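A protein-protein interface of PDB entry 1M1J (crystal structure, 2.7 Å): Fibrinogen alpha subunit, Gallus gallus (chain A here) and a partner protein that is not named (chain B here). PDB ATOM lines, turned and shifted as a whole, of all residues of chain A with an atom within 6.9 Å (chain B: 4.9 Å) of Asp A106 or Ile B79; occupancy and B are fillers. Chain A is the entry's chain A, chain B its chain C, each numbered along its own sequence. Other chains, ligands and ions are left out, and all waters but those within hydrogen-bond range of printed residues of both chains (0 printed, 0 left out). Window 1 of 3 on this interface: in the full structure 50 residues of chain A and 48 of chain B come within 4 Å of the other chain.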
ATOM      1  N   GLY A 101     -10.350 -33.678  19.154  1.00  0.00           N
ATOM      2  CA  GLY A 101      -9.688 -32.626  19.896  1.00  0.00           C
ATOM      3  C   GLY A 101      -8.313 -32.363  19.324  1.00  0.00           C
ATOM      4  O   GLY A 101      -7.949 -31.215  19.075  1.00  0.00           O
ATOM      5  N   ALA A 102      -7.549 -33.433  19.113  1.00  0.00           N
ATOM      6  CA  ALA A 102      -6.205 -33.322  18.557  1.00  0.00           C
ATOM      7  C   ALA A 102      -6.256 -32.383  17.362  1.00  0.00           C
ATOM      8  O   ALA A 102      -5.300 -31.663  17.080  1.00  0.00           O
ATOM      9  CB  ALA A 102      -5.699 -34.693  18.129  1.00  0.00           C
ATOM     10  N   GLN A 103      -7.385 -32.398  16.665  1.00  0.00           N
ATOM     11  CA  GLN A 103      -7.585 -31.537  15.514  1.00  0.00           C
ATOM     12  C   GLN A 103      -7.638 -30.101  16.013  1.00  0.00           C
ATOM     13  O   GLN A 103      -6.960 -29.224  15.480  1.00  0.00           O
ATOM     14  CB  GLN A 103      -8.898 -31.899  14.814  1.00  0.00           C
ATOM     15  CG  GLN A 103      -9.373 -30.902  13.766  1.00  0.00           C
ATOM     16  CD  GLN A 103      -8.330 -30.628  12.703  1.00  0.00           C
ATOM     17  OE1 GLN A 103      -7.708 -31.549  12.172  1.00  0.00           O
ATOM     18  NE2 GLN A 103      -8.140 -29.354  12.378  1.00  0.00           N
ATOM     19  N   GLN A 104      -8.436 -29.875  17.054  1.00  0.00           N
ATOM     20  CA  GLN A 104      -8.592 -28.546  17.633  1.00  0.00           C
ATOM     21  C   GLN A 104      -7.258 -27.954  18.093  1.00  0.00           C
ATOM     22  O   GLN A 104      -7.041 -26.747  17.976  1.00  0.00           O
ATOM     23  CB  GLN A 104      -9.576 -28.589  18.801  1.00  0.00           C
ATOM     24  CG  GLN A 104      -9.933 -27.219  19.367  1.00  0.00           C
ATOM     25  CD  GLN A 104     -10.535 -26.279  18.326  1.00  0.00           C
ATOM     26  OE1 GLN A 104      -9.838 -25.783  17.438  1.00  0.00           O
ATOM     27  NE2 GLN A 104     -11.840 -26.037  18.433  1.00  0.00           N
ATOM     28  N   LEU A 105      -6.371 -28.796  18.619  1.00  0.00           N
ATOM     29  CA  LEU A 105      -5.062 -28.324  19.055  1.00  0.00           C
ATOM     30  C   LEU A 105      -4.285 -27.799  17.855  1.00  0.00           C
ATOM     31  O   LEU A 105      -3.857 -26.647  17.844  1.00  0.00           O
ATOM     32  CB  LEU A 105      -4.259 -29.443  19.722  1.00  0.00           C
ATOM     33  CG  LEU A 105      -4.774 -29.946  21.072  1.00  0.00           C
ATOM     34  CD1 LEU A 105      -3.723 -30.848  21.702  1.00  0.00           C
ATOM     35  CD2 LEU A 105      -5.077 -28.768  21.987  1.00  0.00           C
ATOM     36  N   ASP A 106      -4.102 -28.652  16.850  1.00  0.00           N
ATOM     37  CA  ASP A 106      -3.388 -28.260  15.643  1.00  0.00           C
ATOM     38  C   ASP A 106      -4.026 -27.010  15.068  1.00  0.00           C
ATOM     39  O   ASP A 106      -3.342 -26.145  14.518  1.00  0.00           O
ATOM     40  CB  ASP A 106      -3.423 -29.378  14.602  1.00  0.00           C
ATOM     41  CG  ASP A 106      -2.502 -30.525  14.950  1.00  0.00           C
ATOM     42  OD1 ASP A 106      -1.329 -30.256  15.281  1.00  0.00           O
ATOM     43  OD2 ASP A 106      -2.944 -31.695  14.886  1.00  0.00           O
ATOM     44  N   GLU A 107      -5.346 -26.924  15.209  1.00  0.00           N
ATOM     45  CA  GLU A 107      -6.109 -25.784  14.720  1.00  0.00           C
ATOM     46  C   GLU A 107      -5.638 -24.511  15.423  1.00  0.00           C
ATOM     47  O   GLU A 107      -5.239 -23.545  14.774  1.00  0.00           O
ATOM     48  CB  GLU A 107      -7.601 -26.003  14.998  1.00  0.00           C
ATOM     49  CG  GLU A 107      -8.537 -25.030  14.295  1.00  0.00           C
ATOM     50  CD  GLU A 107      -8.672 -25.321  12.813  1.00  0.00           C
ATOM     51  OE1 GLU A 107      -9.120 -26.435  12.466  1.00  0.00           O
ATOM     52  OE2 GLU A 107      -8.333 -24.439  11.995  1.00  0.00           O
ATOM     53  N   ASN A 108      -5.684 -24.525  16.754  1.00  0.00           N
ATOM     54  CA  ASN A 108      -5.279 -23.379  17.561  1.00  0.00           C
ATOM     55  C   ASN A 108      -3.832 -22.967  17.340  1.00  0.00           C
ATOM     56  O   ASN A 108      -3.553 -21.800  17.062  1.00  0.00           O
ATOM     57  CB  ASN A 108      -5.504 -23.673  19.043  1.00  0.00           C
ATOM     58  CG  ASN A 108      -6.961 -23.937  19.366  1.00  0.00           C
ATOM     59  OD1 ASN A 108      -7.306 -24.249  20.504  1.00  0.00           O
ATOM     60  ND2 ASN A 108      -7.827 -23.809  18.364  1.00  0.00           N
ATOM     61  N   TYR A 109      -2.905 -23.912  17.466  1.00  0.00           N
ATOM     62  CA  TYR A 109      -1.505 -23.577  17.257  1.00  0.00           C
ATOM     63  C   TYR A 109      -1.378 -22.757  15.979  1.00  0.00           C
ATOM     64  O   TYR A 109      -0.494 -21.917  15.856  1.00  0.00           O
ATOM     65  CB  TYR A 109      -0.638 -24.833  17.135  1.00  0.00           C
ATOM     66  CG  TYR A 109       0.831 -24.502  16.995  1.00  0.00           C
ATOM     67  CD1 TYR A 109       1.571 -24.053  18.094  1.00  0.00           C
ATOM     68  CD2 TYR A 109       1.466 -24.561  15.752  1.00  0.00           C
ATOM     69  CE1 TYR A 109       2.909 -23.665  17.962  1.00  0.00           C
ATOM     70  CE2 TYR A 109       2.807 -24.174  15.606  1.00  0.00           C
ATOM     71  CZ  TYR A 109       3.520 -23.725  16.716  1.00  0.00           C
ATOM     72  OH  TYR A 109       4.836 -23.331  16.583  1.00  0.00           O
ATOM     73  N   GLY A 110      -2.282 -23.005  15.036  1.00  0.00           N
ATOM     74  CA  GLY A 110      -2.265 -22.298  13.771  1.00  0.00           C
ATOM     75  C   GLY A 110      -2.510 -20.814  13.918  1.00  0.00           C
ATOM     76  O   GLY A 110      -1.804 -20.002  13.321  1.00  0.00           O
ATOM     77  N   HIS A 111      -3.511 -20.446  14.707  1.00  0.00           N
ATOM     78  CA  HIS A 111      -3.813 -19.036  14.904  1.00  0.00           C
ATOM     79  C   HIS A 111      -2.679 -18.393  15.682  1.00  0.00           C
ATOM     80  O   HIS A 111      -1.997 -17.494  15.182  1.00  0.00           O
ATOM     81  CB  HIS A 111      -5.128 -18.861  15.671  1.00  0.00           C
ATOM     82  CG  HIS A 111      -6.302 -19.520  15.012  1.00  0.00           C
ATOM     83  ND1 HIS A 111      -6.558 -19.406  13.661  1.00  0.00           N
ATOM     84  CD2 HIS A 111      -7.295 -20.289  15.519  1.00  0.00           C
ATOM     85  CE1 HIS A 111      -7.656 -20.077  13.365  1.00  0.00           C
ATOM     86  NE2 HIS A 111      -8.123 -20.623  14.474  1.00  0.00           N
ATOM     87  N   MET A 208       2.046 -27.974   6.572  1.00  0.00           N
ATOM     88  CA  MET A 208       1.242 -28.275   7.757  1.00  0.00           C
ATOM     89  C   MET A 208      -0.226 -28.329   7.325  1.00  0.00           C
ATOM     90  O   MET A 208      -0.868 -27.291   7.149  1.00  0.00           O
ATOM     91  CB  MET A 208       1.446 -27.185   8.823  1.00  0.00           C
ATOM     92  CG  MET A 208       1.480 -27.673  10.285  1.00  0.00           C
ATOM     93  SD  MET A 208      -0.126 -27.944  11.102  1.00  0.00           S
ATOM     94  CE  MET A 208      -0.460 -26.307  11.794  1.00  0.00           C
ATOM     95  N   ARG A 209      -0.742 -29.543   7.139  1.00  0.00           N
ATOM     96  CA  ARG A 209      -2.132 -29.757   6.727  1.00  0.00           C
ATOM     97  C   ARG A 209      -2.878 -30.603   7.759  1.00  0.00           C
ATOM     98  O   ARG A 209      -2.333 -31.578   8.279  1.00  0.00           O
ATOM     99  CB  ARG A 209      -2.176 -30.459   5.366  1.00  0.00           C
ATOM    100  CG  ARG A 209      -1.613 -29.631   4.228  1.00  0.00           C
ATOM    101  CD  ARG A 209      -1.275 -30.500   3.028  1.00  0.00           C
ATOM    102  NE  ARG A 209      -0.256 -31.499   3.350  1.00  0.00           N
ATOM    103  CZ  ARG A 209       0.350 -32.273   2.454  1.00  0.00           C
ATOM    104  NH1 ARG A 209       0.044 -32.170   1.166  1.00  0.00           N
ATOM    105  NH2 ARG A 209       1.265 -33.151   2.844  1.00  0.00           N
ATOM    106  N   PRO A 210      -4.139 -30.242   8.064  1.00  0.00           N
ATOM    107  CA  PRO A 210      -4.955 -30.976   9.041  1.00  0.00           C
ATOM    108  C   PRO A 210      -4.894 -32.500   8.873  1.00  0.00           C
ATOM    109  O   PRO A 210      -4.027 -33.157   9.454  1.00  0.00           O
ATOM    110  CB  PRO A 210      -6.352 -30.407   8.807  1.00  0.00           C
ATOM    111  CG  PRO A 210      -6.055 -28.973   8.476  1.00  0.00           C
ATOM    112  CD  PRO A 210      -4.896 -29.106   7.503  1.00  0.00           C
ATOM    113  N   GLN B  77       8.215 -31.564  24.383  1.00  0.00           N
ATOM    114  CA  GLN B  77       7.172 -30.555  24.196  1.00  0.00           C
ATOM    115  C   GLN B  77       6.178 -30.926  23.088  1.00  0.00           C
ATOM    116  O   GLN B  77       6.546 -31.047  21.917  1.00  0.00           O
ATOM    117  CB  GLN B  77       7.806 -29.186  23.908  1.00  0.00           C
ATOM    118  CG  GLN B  77       8.739 -28.692  25.019  1.00  0.00           C
ATOM    119  CD  GLN B  77       9.298 -27.300  24.755  1.00  0.00           C
ATOM    120  OE1 GLN B  77       9.843 -27.031  23.684  1.00  0.00           O
ATOM    121  NE2 GLN B  77       9.170 -26.412  25.738  1.00  0.00           N
ATOM    122  N   SER B  78       4.918 -31.107  23.479  1.00  0.00           N
ATOM    123  CA  SER B  78       3.850 -31.469  22.550  1.00  0.00           C
ATOM    124  C   SER B  78       3.349 -30.237  21.806  1.00  0.00           C
ATOM    125  O   SER B  78       4.127 -29.347  21.472  1.00  0.00           O
ATOM    126  CB  SER B  78       2.691 -32.119  23.315  1.00  0.00           C
ATOM    127  OG  SER B  78       1.675 -32.570  22.434  1.00  0.00           O
ATOM    128  N   ILE B  79       2.046 -30.192  21.542  1.00  0.00           N
ATOM    129  CA  ILE B  79       1.447 -29.058  20.849  1.00  0.00           C
ATOM    130  C   ILE B  79       0.960 -28.022  21.852  1.00  0.00           C
ATOM    131  O   ILE B  79       1.356 -26.859  21.787  1.00  0.00           O
ATOM    132  CB  ILE B  79       0.260 -29.500  19.950  1.00  0.00           C
ATOM    133  CG1 ILE B  79       0.790 -30.193  18.696  1.00  0.00           C
ATOM    134  CG2 ILE B  79      -0.591 -28.297  19.552  1.00  0.00           C
ATOM    135  CD1 ILE B  79       1.616 -29.289  17.806  1.00  0.00           C
ATOM    136  N   GLU B  80       0.108 -28.442  22.784  1.00  0.00           N
ATOM    137  CA  GLU B  80      -0.415 -27.518  23.786  1.00  0.00           C
ATOM    138  C   GLU B  80       0.752 -26.908  24.548  1.00  0.00           C
ATOM    139  O   GLU B  80       0.597 -25.923  25.268  1.00  0.00           O
ATOM    140  CB  GLU B  80      -1.355 -28.242  24.757  1.00  0.00           C
ATOM    141  CG  GLU B  80      -2.281 -27.299  25.522  1.00  0.00           C
ATOM    142  CD  GLU B  80      -3.263 -28.028  26.426  1.00  0.00           C
ATOM    143  OE1 GLU B  80      -3.968 -28.936  25.935  1.00  0.00           O
ATOM    144  OE2 GLU B  80      -3.338 -27.686  27.627  1.00  0.00           O
ATOM    145  N   GLN B  81       1.927 -27.505  24.375  1.00  0.00           N
ATOM    146  CA  GLN B  81       3.134 -27.030  25.029  1.00  0.00           C
ATOM    147  C   GLN B  81       3.796 -25.958  24.168  1.00  0.00           C
ATOM    148  O   GLN B  81       4.336 -24.984  24.686  1.00  0.00           O
ATOM    149  CB  GLN B  81       4.085 -28.204  25.262  1.00  0.00           C
ATOM    150  CG  GLN B  81       3.476 -29.290  26.139  1.00  0.00           C
ATOM    151  CD  GLN B  81       4.389 -30.486  26.325  1.00  0.00           C
ATOM    152  OE1 GLN B  81       5.537 -30.347  26.754  1.00  0.00           O
ATOM    153  NE2 GLN B  81       3.878 -31.676  26.010  1.00  0.00           N
ATOM    154  N   LEU B  82       3.741 -26.144  22.851  1.00  0.00           N
ATOM    155  CA  LEU B  82       4.311 -25.185  21.913  1.00  0.00           C
ATOM    156  C   LEU B  82       3.389 -23.978  21.737  1.00  0.00           C
ATOM    157  O   LEU B  82       3.835 -22.907  21.319  1.00  0.00           O
ATOM    158  CB  LEU B  82       4.540 -25.837  20.546  1.00  0.00           C
ATOM    159  CG  LEU B  82       5.726 -26.784  20.341  1.00  0.00           C
ATOM    160  CD1 LEU B  82       5.664 -27.375  18.936  1.00  0.00           C
ATOM    161  CD2 LEU B  82       7.029 -26.031  20.533  1.00  0.00           C
ATOM    162  N   THR B  83       2.107 -24.154  22.050  1.00  0.00           N
ATOM    163  CA  THR B  83       1.133 -23.075  21.919  1.00  0.00           C
ATOM    164  C   THR B  83       1.180 -22.111  23.103  1.00  0.00           C
ATOM    165  O   THR B  83       1.147 -20.897  22.912  1.00  0.00           O
ATOM    166  CB  THR B  83      -0.306 -23.610  21.780  1.00  0.00           C
ATOM    167  OG1 THR B  83      -0.724 -24.197  23.019  1.00  0.00           O
ATOM    168  CG2 THR B  83      -0.378 -24.644  20.675  1.00  0.00           C
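Printed residues of chain A within 4 Å of Ile B79: Leu A105 (3.8 Å) and Asp A106 (3.998 Å).
Of the printed residues of chain B, Leu A105 touches Ile B79 (3.8 Å).
Of the printed residues of chain A, Leu B82 touches Tyr A109.
Of the printed residues of chain A, Thr B83 touches Tyr A109 (3.3 Å).
Of the printed residues of chain B, Tyr A109 touches Leu B82 and Thr B83.
Glu A107 touches none of the printed residues of chain B.
Gln A103 touches none of the printed residues of chain B.
The nearest printed residue of chain B that does not touch Asp A106 is Thr B83 (6.7 Å).
O of Glu B80 is in hydrogen-bond range of OG1 of Thr B83 (3.1 Å).
Leu A105 touches Ile B79 (CB to CG2, 3.8 Å).
Asp A106 touches Ile B79 (OD1 to CD1, 3.998 Å).
Leu B82 touches Tyr A109 (O to CE1, 3.6 Å).
Thr B83 touches Tyr A109.
Of the 14 printed residues of chain A, 3 touch a printed residue of chain B.
Among the printed residues, 4 pairs touch across the chains.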
